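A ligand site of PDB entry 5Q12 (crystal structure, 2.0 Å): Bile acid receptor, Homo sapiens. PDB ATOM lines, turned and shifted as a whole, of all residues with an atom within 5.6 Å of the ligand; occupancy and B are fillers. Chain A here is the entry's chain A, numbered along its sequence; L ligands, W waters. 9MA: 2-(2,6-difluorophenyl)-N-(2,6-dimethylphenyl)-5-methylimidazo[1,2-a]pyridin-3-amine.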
ATOM      1  N   PHE A  45     -27.988 -25.900   0.559  1.00  0.00           N
ATOM      2  CA  PHE A  45     -28.156 -25.346   1.909  1.00  0.00           C
ATOM      3  C   PHE A  45     -28.987 -26.261   2.823  1.00  0.00           C
ATOM      4  O   PHE A  45     -28.707 -26.353   4.025  1.00  0.00           O
ATOM      5  CB  PHE A  45     -28.700 -23.924   1.870  1.00  0.00           C
ATOM      6  CG  PHE A  45     -28.546 -23.220   3.195  1.00  0.00           C
ATOM      7  CD1 PHE A  45     -27.349 -22.587   3.529  1.00  0.00           C
ATOM      8  CD2 PHE A  45     -29.585 -23.202   4.122  1.00  0.00           C
ATOM      9  CE1 PHE A  45     -27.209 -21.932   4.752  1.00  0.00           C
ATOM     10  CE2 PHE A  45     -29.429 -22.564   5.363  1.00  0.00           C
ATOM     11  CZ  PHE A  45     -28.256 -21.916   5.651  1.00  0.00           C
ATOM     12  N   LEU A  48     -26.666 -28.783   4.303  1.00  0.00           N
ATOM     13  CA  LEU A  48     -25.888 -28.122   5.365  1.00  0.00           C
ATOM     14  C   LEU A  48     -26.735 -27.920   6.629  1.00  0.00           C
ATOM     15  O   LEU A  48     -26.190 -27.997   7.737  1.00  0.00           O
ATOM     16  CB  LEU A  48     -25.306 -26.779   4.887  1.00  0.00           C
ATOM     17  CG  LEU A  48     -24.439 -26.788   3.597  1.00  0.00           C
ATOM     18  CD1 LEU A  48     -23.763 -25.440   3.386  1.00  0.00           C
ATOM     19  CD2 LEU A  48     -23.385 -27.900   3.627  1.00  0.00           C
ATOM     20  N   THR A  49     -28.054 -27.688   6.472  1.00  0.00           N
ATOM     21  CA  THR A  49     -29.002 -27.530   7.599  1.00  0.00           C
ATOM     22  C   THR A  49     -29.117 -28.865   8.344  1.00  0.00           C
ATOM     23  O   THR A  49     -29.034 -28.892   9.563  1.00  0.00           O
ATOM     24  CB  THR A  49     -30.356 -26.965   7.111  1.00  0.00           C
ATOM     25  OG1 THR A  49     -30.106 -25.699   6.508  1.00  0.00           O
ATOM     26  CG2 THR A  49     -31.377 -26.784   8.243  1.00  0.00           C
ATOM     27  N   MET A  51     -26.892 -31.266   8.300  1.00  0.00           N
ATOM     28  CA  MET A  51     -25.593 -31.547   8.910  1.00  0.00           C
ATOM     29  C   MET A  51     -25.447 -30.764  10.196  1.00  0.00           C
ATOM     30  O   MET A  51     -25.014 -31.331  11.192  1.00  0.00           O
ATOM     31  CB  MET A  51     -24.462 -31.235   7.926  1.00  0.00           C
ATOM     32  CG  MET A  51     -24.319 -32.288   6.877  1.00  0.00           C
ATOM     33  SD  MET A  51     -22.988 -31.881   5.731  1.00  0.00           S
ATOM     34  CE  MET A  51     -22.214 -33.444   5.601  1.00  0.00           C
ATOM     35  N   ALA A  52     -25.834 -29.476  10.171  1.00  0.00           N
ATOM     36  CA  ALA A  52     -25.767 -28.582  11.332  1.00  0.00           C
ATOM     37  C   ALA A  52     -26.620 -29.087  12.498  1.00  0.00           C
ATOM     38  O   ALA A  52     -26.129 -29.048  13.621  1.00  0.00           O
ATOM     39  CB  ALA A  52     -26.165 -27.165  10.939  1.00  0.00           C
ATOM     40  N   HIS A  55     -24.846 -32.009  13.997  1.00  0.00           N
ATOM     41  CA  HIS A  55     -23.714 -31.487  14.772  1.00  0.00           C
ATOM     42  C   HIS A  55     -24.152 -31.050  16.180  1.00  0.00           C
ATOM     43  O   HIS A  55     -23.436 -31.283  17.151  1.00  0.00           O
ATOM     44  CB  HIS A  55     -23.034 -30.295  14.068  1.00  0.00           C
ATOM     45  CG  HIS A  55     -22.127 -30.677  12.932  1.00  0.00           C
ATOM     46  ND1 HIS A  55     -21.061 -31.530  13.125  1.00  0.00           N
ATOM     47  CD2 HIS A  55     -22.145 -30.285  11.632  1.00  0.00           C
ATOM     48  CE1 HIS A  55     -20.482 -31.656  11.935  1.00  0.00           C
ATOM     49  NE2 HIS A  55     -21.098 -30.933  11.012  1.00  0.00           N
ATOM     50  N   MET A  89     -18.664 -27.554  16.713  1.00  0.00           N
ATOM     51  CA  MET A  89     -19.283 -27.809  15.406  1.00  0.00           C
ATOM     52  C   MET A  89     -18.239 -27.666  14.289  1.00  0.00           C
ATOM     53  O   MET A  89     -18.137 -28.562  13.448  1.00  0.00           O
ATOM     54  CB  MET A  89     -20.456 -26.843  15.140  1.00  0.00           C
ATOM     55  CG  MET A  89     -21.718 -27.161  15.941  1.00  0.00           C
ATOM     56  SD  MET A  89     -22.966 -25.827  15.924  1.00  0.00           S
ATOM     57  CE  MET A  89     -23.569 -25.963  14.228  1.00  0.00           C
ATOM     58  N   PHE A  90     -17.435 -26.552  14.300  1.00  0.00           N
ATOM     59  CA  PHE A  90     -16.383 -26.353  13.288  1.00  0.00           C
ATOM     60  C   PHE A  90     -15.333 -27.466  13.364  1.00  0.00           C
ATOM     61  O   PHE A  90     -14.950 -28.014  12.327  1.00  0.00           O
ATOM     62  CB  PHE A  90     -15.741 -24.947  13.409  1.00  0.00           C
ATOM     63  CG  PHE A  90     -16.368 -23.861  12.560  1.00  0.00           C
ATOM     64  CD1 PHE A  90     -17.419 -23.091  13.048  1.00  0.00           C
ATOM     65  CD2 PHE A  90     -15.908 -23.608  11.269  1.00  0.00           C
ATOM     66  CE1 PHE A  90     -18.007 -22.084  12.259  1.00  0.00           C
ATOM     67  CE2 PHE A  90     -16.512 -22.617  10.479  1.00  0.00           C
ATOM     68  CZ  PHE A  90     -17.538 -21.842  10.988  1.00  0.00           C
ATOM     69  N   SER A  93     -16.858 -30.709  12.010  1.00  0.00           N
ATOM     70  CA  SER A  93     -17.024 -30.591  10.559  1.00  0.00           C
ATOM     71  C   SER A  93     -15.706 -30.815   9.807  1.00  0.00           C
ATOM     72  O   SER A  93     -15.743 -31.358   8.702  1.00  0.00           O
ATOM     73  CB  SER A  93     -17.686 -29.272  10.177  1.00  0.00           C
ATOM     74  OG  SER A  93     -16.797 -28.181  10.284  1.00  0.00           O
ATOM     75  N   ILE A 113     -21.088 -26.750  -0.582  1.00  0.00           N
ATOM     76  CA  ILE A 113     -20.787 -25.663   0.363  1.00  0.00           C
ATOM     77  C   ILE A 113     -20.508 -24.368  -0.406  1.00  0.00           C
ATOM     78  O   ILE A 113     -21.068 -23.321  -0.060  1.00  0.00           O
ATOM     79  CB  ILE A 113     -19.629 -26.056   1.333  1.00  0.00           C
ATOM     80  CG1 ILE A 113     -20.090 -27.127   2.333  1.00  0.00           C
ATOM     81  CG2 ILE A 113     -19.070 -24.812   2.074  1.00  0.00           C
ATOM     82  CD1 ILE A 113     -19.010 -27.800   3.168  1.00  0.00           C
ATOM     83  N   ILE A 118     -23.465 -18.756   0.132  1.00  0.00           N
ATOM     84  CA  ILE A 118     -22.751 -18.204   1.280  1.00  0.00           C
ATOM     85  C   ILE A 118     -21.524 -17.468   0.756  1.00  0.00           C
ATOM     86  O   ILE A 118     -20.787 -18.015  -0.060  1.00  0.00           O
ATOM     87  CB  ILE A 118     -22.356 -19.281   2.330  1.00  0.00           C
ATOM     88  CG1 ILE A 118     -23.588 -20.098   2.794  1.00  0.00           C
ATOM     89  CG2 ILE A 118     -21.629 -18.637   3.534  1.00  0.00           C
ATOM     90  CD1 ILE A 118     -23.265 -21.405   3.490  1.00  0.00           C
ATOM     91  N   ILE A 123     -16.572 -18.751   3.716  1.00  0.00           N
ATOM     92  CA  ILE A 123     -16.215 -20.056   3.152  1.00  0.00           C
ATOM     93  C   ILE A 123     -14.687 -20.257   3.090  1.00  0.00           C
ATOM     94  O   ILE A 123     -14.199 -21.337   3.441  1.00  0.00           O
ATOM     95  CB  ILE A 123     -16.939 -20.274   1.778  1.00  0.00           C
ATOM     96  CG1 ILE A 123     -18.495 -20.370   1.934  1.00  0.00           C
ATOM     97  CG2 ILE A 123     -16.384 -21.450   0.976  1.00  0.00           C
ATOM     98  CD1 ILE A 123     -19.058 -21.308   3.088  1.00  0.00           C
ATOM     99  N   MET A 126     -12.973 -21.285   6.429  1.00  0.00           N
ATOM    100  CA  MET A 126     -13.420 -22.641   6.772  1.00  0.00           C
ATOM    101  C   MET A 126     -12.510 -23.692   6.131  1.00  0.00           C
ATOM    102  O   MET A 126     -11.946 -24.499   6.861  1.00  0.00           O
ATOM    103  CB  MET A 126     -14.876 -22.819   6.328  1.00  0.00           C
ATOM    104  CG  MET A 126     -15.555 -24.010   6.913  1.00  0.00           C
ATOM    105  SD  MET A 126     -17.255 -24.126   6.293  1.00  0.00           S
ATOM    106  CE  MET A 126     -17.936 -22.555   6.846  1.00  0.00           C
ATOM    107  N   TYR A 130      -9.701 -26.344   7.616  1.00  0.00           N
ATOM    108  CA  TYR A 130      -9.738 -27.768   7.288  1.00  0.00           C
ATOM    109  C   TYR A 130      -8.356 -28.234   6.807  1.00  0.00           C
ATOM    110  O   TYR A 130      -7.907 -29.298   7.227  1.00  0.00           O
ATOM    111  CB  TYR A 130     -10.791 -28.080   6.216  1.00  0.00           C
ATOM    112  CG  TYR A 130     -12.248 -27.935   6.623  1.00  0.00           C
ATOM    113  CD1 TYR A 130     -12.599 -27.636   7.940  1.00  0.00           C
ATOM    114  CD2 TYR A 130     -13.260 -28.086   5.691  1.00  0.00           C
ATOM    115  CE1 TYR A 130     -13.937 -27.487   8.311  1.00  0.00           C
ATOM    116  CE2 TYR A 130     -14.597 -27.949   6.055  1.00  0.00           C
ATOM    117  CZ  TYR A 130     -14.931 -27.659   7.361  1.00  0.00           C
ATOM    118  OH  TYR A 130     -16.257 -27.536   7.708  1.00  0.00           O
ATOM    119  N   HIS A 208     -18.892 -16.774  12.286  1.00  0.00           N
ATOM    120  CA  HIS A 208     -20.185 -17.478  12.287  1.00  0.00           C
ATOM    121  C   HIS A 208     -21.338 -16.531  12.646  1.00  0.00           C
ATOM    122  O   HIS A 208     -22.389 -16.575  12.013  1.00  0.00           O
ATOM    123  CB  HIS A 208     -20.138 -18.673  13.242  1.00  0.00           C
ATOM    124  CG  HIS A 208     -21.288 -19.614  13.077  1.00  0.00           C
ATOM    125  ND1 HIS A 208     -22.431 -19.486  13.835  1.00  0.00           N
ATOM    126  CD2 HIS A 208     -21.436 -20.664  12.231  1.00  0.00           C
ATOM    127  CE1 HIS A 208     -23.234 -20.455  13.444  1.00  0.00           C
ATOM    128  NE2 HIS A 208     -22.676 -21.192  12.479  1.00  0.00           N
ATOM    129  N   MET A 211     -21.855 -14.231   9.745  1.00  0.00           N
ATOM    130  CA  MET A 211     -22.439 -15.055   8.681  1.00  0.00           C
ATOM    131  C   MET A 211     -23.966 -15.094   8.854  1.00  0.00           C
ATOM    132  O   MET A 211     -24.700 -14.757   7.925  1.00  0.00           O
ATOM    133  CB  MET A 211     -21.864 -16.478   8.740  1.00  0.00           C
ATOM    134  CG  MET A 211     -22.013 -17.265   7.464  1.00  0.00           C
ATOM    135  SD  MET A 211     -21.841 -19.053   7.675  1.00  0.00           S
ATOM    136  CE  MET A 211     -20.155 -19.193   8.346  1.00  0.00           C
ATOM    137  N   LEU A 212     -24.442 -15.494  10.057  1.00  0.00           N
ATOM    138  CA  LEU A 212     -25.869 -15.580  10.374  1.00  0.00           C
ATOM    139  C   LEU A 212     -26.604 -14.259  10.199  1.00  0.00           C
ATOM    140  O   LEU A 212     -27.705 -14.249   9.667  1.00  0.00           O
ATOM    141  CB  LEU A 212     -26.115 -16.143  11.786  1.00  0.00           C
ATOM    142  CG  LEU A 212     -25.639 -17.566  12.067  1.00  0.00           C
ATOM    143  CD1 LEU A 212     -25.991 -17.987  13.471  1.00  0.00           C
ATOM    144  CD2 LEU A 212     -26.216 -18.548  11.115  1.00  0.00           C
ATOM    145  N   TRP A 215     -27.541 -13.152   6.484  1.00  0.00           N
ATOM    146  CA  TRP A 215     -28.699 -13.791   5.873  1.00  0.00           C
ATOM    147  C   TRP A 215     -29.966 -13.087   6.392  1.00  0.00           C
ATOM    148  O   TRP A 215     -30.158 -12.992   7.603  1.00  0.00           O
ATOM    149  CB  TRP A 215     -28.721 -15.307   6.197  1.00  0.00           C
ATOM    150  CG  TRP A 215     -27.454 -16.066   5.896  1.00  0.00           C
ATOM    151  CD1 TRP A 215     -26.500 -15.744   4.986  1.00  0.00           C
ATOM    152  CD2 TRP A 215     -27.066 -17.327   6.458  1.00  0.00           C
ATOM    153  NE1 TRP A 215     -25.514 -16.709   4.974  1.00  0.00           N
ATOM    154  CE2 TRP A 215     -25.841 -17.697   5.869  1.00  0.00           C
ATOM    155  CE3 TRP A 215     -27.632 -18.177   7.437  1.00  0.00           C
ATOM    156  CZ2 TRP A 215     -25.173 -18.875   6.203  1.00  0.00           C
ATOM    157  CZ3 TRP A 215     -26.961 -19.351   7.761  1.00  0.00           C
ATOM    158  CH2 TRP A 215     -25.738 -19.674   7.163  1.00  0.00           C
ATOM    159  N   LYS A 221     -31.778 -19.129   3.341  1.00  0.00           N
ATOM    160  CA  LYS A 221     -30.761 -19.485   4.328  1.00  0.00           C
ATOM    161  C   LYS A 221     -31.160 -19.211   5.772  1.00  0.00           C
ATOM    162  O   LYS A 221     -30.556 -19.782   6.697  1.00  0.00           O
ATOM    163  CB  LYS A 221     -29.408 -18.815   4.015  1.00  0.00           C
ATOM    164  CG  LYS A 221     -28.791 -19.276   2.704  1.00  0.00           C
ATOM    165  CD  LYS A 221     -27.435 -18.602   2.442  1.00  0.00           C
ATOM    166  CE  LYS A 221     -27.558 -17.183   1.938  1.00  0.00           C
ATOM    167  NZ  LYS A 221     -28.189 -17.122   0.584  1.00  0.00           N
ATOM    168  N   THR A 223     -32.641 -19.812   8.949  1.00  0.00           N
ATOM    169  CA  THR A 223     -33.094 -21.053   9.581  1.00  0.00           C
ATOM    170  C   THR A 223     -33.275 -20.810  11.081  1.00  0.00           C
ATOM    171  O   THR A 223     -32.314 -20.960  11.849  1.00  0.00           O
ATOM    172  CB  THR A 223     -32.122 -22.208   9.254  1.00  0.00           C
ATOM    173  OG1 THR A 223     -30.803 -21.815   9.627  1.00  0.00           O
ATOM    174  CG2 THR A 223     -32.131 -22.578   7.781  1.00  0.00           C
ATOM    175  N   LEU A 226     -31.745 -23.138  14.097  1.00  0.00           N
ATOM    176  CA  LEU A 226     -30.320 -23.000  14.391  1.00  0.00           C
ATOM    177  C   LEU A 226     -29.917 -21.592  14.767  1.00  0.00           C
ATOM    178  O   LEU A 226     -29.233 -21.412  15.764  1.00  0.00           O
ATOM    179  CB  LEU A 226     -29.463 -23.525  13.242  1.00  0.00           C
ATOM    180  CG  LEU A 226     -29.591 -25.005  12.915  1.00  0.00           C
ATOM    181  CD1 LEU A 226     -29.225 -25.274  11.487  1.00  0.00           C
ATOM    182  CD2 LEU A 226     -28.774 -25.864  13.877  1.00  0.00           C
ATOM    183  N   CYS A 227     -30.351 -20.581  13.977  1.00  0.00           N
ATOM    184  CA  CYS A 227     -30.009 -19.182  14.187  1.00  0.00           C
ATOM    185  C   CYS A 227     -30.396 -18.636  15.565  1.00  0.00           C
ATOM    186  O   CYS A 227     -29.627 -17.857  16.134  1.00  0.00           O
ATOM    187  CB  CYS A 227     -30.551 -18.309  13.061  1.00  0.00           C
ATOM    188  SG  CYS A 227     -29.851 -18.702  11.432  1.00  0.00           S
ATOM    189  N   TRP A 230     -28.155 -18.652  18.886  1.00  0.00           N
ATOM    190  CA  TRP A 230     -27.259 -17.504  19.097  1.00  0.00           C
ATOM    191  C   TRP A 230     -27.960 -16.121  19.122  1.00  0.00           C
ATOM    192  O   TRP A 230     -27.335 -15.141  19.528  1.00  0.00           O
ATOM    193  CB  TRP A 230     -26.126 -17.524  18.054  1.00  0.00           C
ATOM    194  CG  TRP A 230     -25.302 -18.764  18.123  1.00  0.00           C
ATOM    195  CD1 TRP A 230     -24.317 -19.044  19.026  1.00  0.00           C
ATOM    196  CD2 TRP A 230     -25.440 -19.950  17.321  1.00  0.00           C
ATOM    197  NE1 TRP A 230     -23.820 -20.304  18.824  1.00  0.00           N
ATOM    198  CE2 TRP A 230     -24.485 -20.887  17.767  1.00  0.00           C
ATOM    199  CE3 TRP A 230     -26.284 -20.304  16.250  1.00  0.00           C
ATOM    200  CZ2 TRP A 230     -24.341 -22.152  17.190  1.00  0.00           C
ATOM    201  CZ3 TRP A 230     -26.113 -21.550  15.656  1.00  0.00           C
ATOM    202  CH2 TRP A 230     -25.172 -22.464  16.134  1.00  0.00           C
HETATM  203  N3  9MA L   1     -24.119 -25.415   8.190  1.00  0.00           N
HETATM  204  C4  9MA L   1     -26.122 -22.204  11.195  1.00  0.00           C
HETATM  205  C5  9MA L   1     -25.114 -23.081  10.705  1.00  0.00           C
HETATM  206  C7  9MA L   1     -26.640 -23.661   8.824  1.00  0.00           C
HETATM  207  C8  9MA L   1     -27.567 -22.806   9.336  1.00  0.00           C
HETATM  208  C13 9MA L   1     -22.481 -24.120   6.856  1.00  0.00           C
HETATM  209  C15 9MA L   1     -20.558 -25.258   5.907  1.00  0.00           C
HETATM  210  C17 9MA L   1     -21.302 -24.105   6.107  1.00  0.00           C
HETATM  211  C20 9MA L   1     -22.034 -24.855  10.432  1.00  0.00           C
HETATM  212  C21 9MA L   1     -21.823 -26.167  10.843  1.00  0.00           C
HETATM  213  C22 9MA L   1     -20.876 -24.124  10.158  1.00  0.00           C
HETATM  214  C26 9MA L   1     -19.608 -24.641  10.269  1.00  0.00           C
HETATM  215  C19 9MA L   1     -22.574 -27.884   7.783  1.00  0.00           C
HETATM  216  C14 9MA L   1     -22.144 -26.548   7.210  1.00  0.00           C
HETATM  217  C16 9MA L   1     -20.973 -26.464   6.451  1.00  0.00           C
HETATM  218  C18 9MA L   1     -23.259 -22.836   7.051  1.00  0.00           C
HETATM  219  C12 9MA L   1     -22.899 -25.360   7.404  1.00  0.00           C
HETATM  220  C2  9MA L   1     -24.266 -24.569   9.262  1.00  0.00           C
HETATM  221  C1  9MA L   1     -23.377 -24.276  10.288  1.00  0.00           C
HETATM  222  N10 9MA L   1     -23.904 -23.362  11.172  1.00  0.00           N
HETATM  223  C9  9MA L   1     -27.314 -22.064  10.533  1.00  0.00           C
HETATM  224  C11 9MA L   1     -26.871 -24.444   7.586  1.00  0.00           C
HETATM  225  N6  9MA L   1     -25.411 -23.783   9.518  1.00  0.00           N
HETATM  226  F24 9MA L   1     -22.908 -26.922  11.112  1.00  0.00           F
HETATM  227  C27 9MA L   1     -20.569 -26.734  10.969  1.00  0.00           C
HETATM  228  C25 9MA L   1     -19.465 -25.953  10.685  1.00  0.00           C
HETATM  229  F23 9MA L   1     -21.026 -22.839   9.760  1.00  0.00           F
HETATM  230  O   HOH W   1     -18.364 -28.631   6.388  1.00  0.00           O
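O of Leu 48 is in hydrogen-bond range of N3 of the ligand.
N10 of the ligand is in hydrogen-bond range of NE2 of His 208 (2.8 Å).
The backbone carbonyl oxygen (O) of Phe 45 lies within hydrogen-bond range of the side-chain hydroxyl (OG1) of Thr 49, 2.9 Å away.
O of Thr 223 is in hydrogen-bond range of SG of Cys 227, at 3.4 Å.
O of Met 89 lies close to OG of Ser 93 (3.5 Å).
OG of Ser 93 sits at hydrogen-bond distance from OH of Tyr 130, at 2.7 Å.
OG of Ser 93 is in hydrogen-bond range of O of Phe 90 (2.8 Å).
Residues that only touch the ligand: Ala 52 (3.3 Å), Met 89 (3.3 Å), Thr 223 (3.4 Å), Phe 45 (3.5 Å), His 55 (3.5 Å), Ser 93 (3.5 Å), Met 126 (3.5 Å), Phe 90 (3.6 Å), Thr 49 (3.6 Å), Leu 212 (3.7 Å), Leu 226 (3.7 Å), Ile 118 (3.8 Å), Trp 215 (3.8 Å) and Met 51 (3.8 Å).
Hydrophobic or aromatic side chains that line the ligand: Phe 45, Leu 48, Met 51, Ala 52, His 55, Met 89, Phe 90, Ile 118, Met 126, His 208, Leu 212, Trp 215 and Leu 226.
16 residues have an atom within 4 Å of the ligand: Phe 45, Leu 48, Thr 49, Met 51, Ala 52, His 55, Met 89, Phe 90, Ser 93, Ile 118, Met 126, His 208, Leu 212, Trp 215, Thr 223 and Leu 226.
Along chain A the residues within 4 Å of the ligand span positions 45 to 226.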
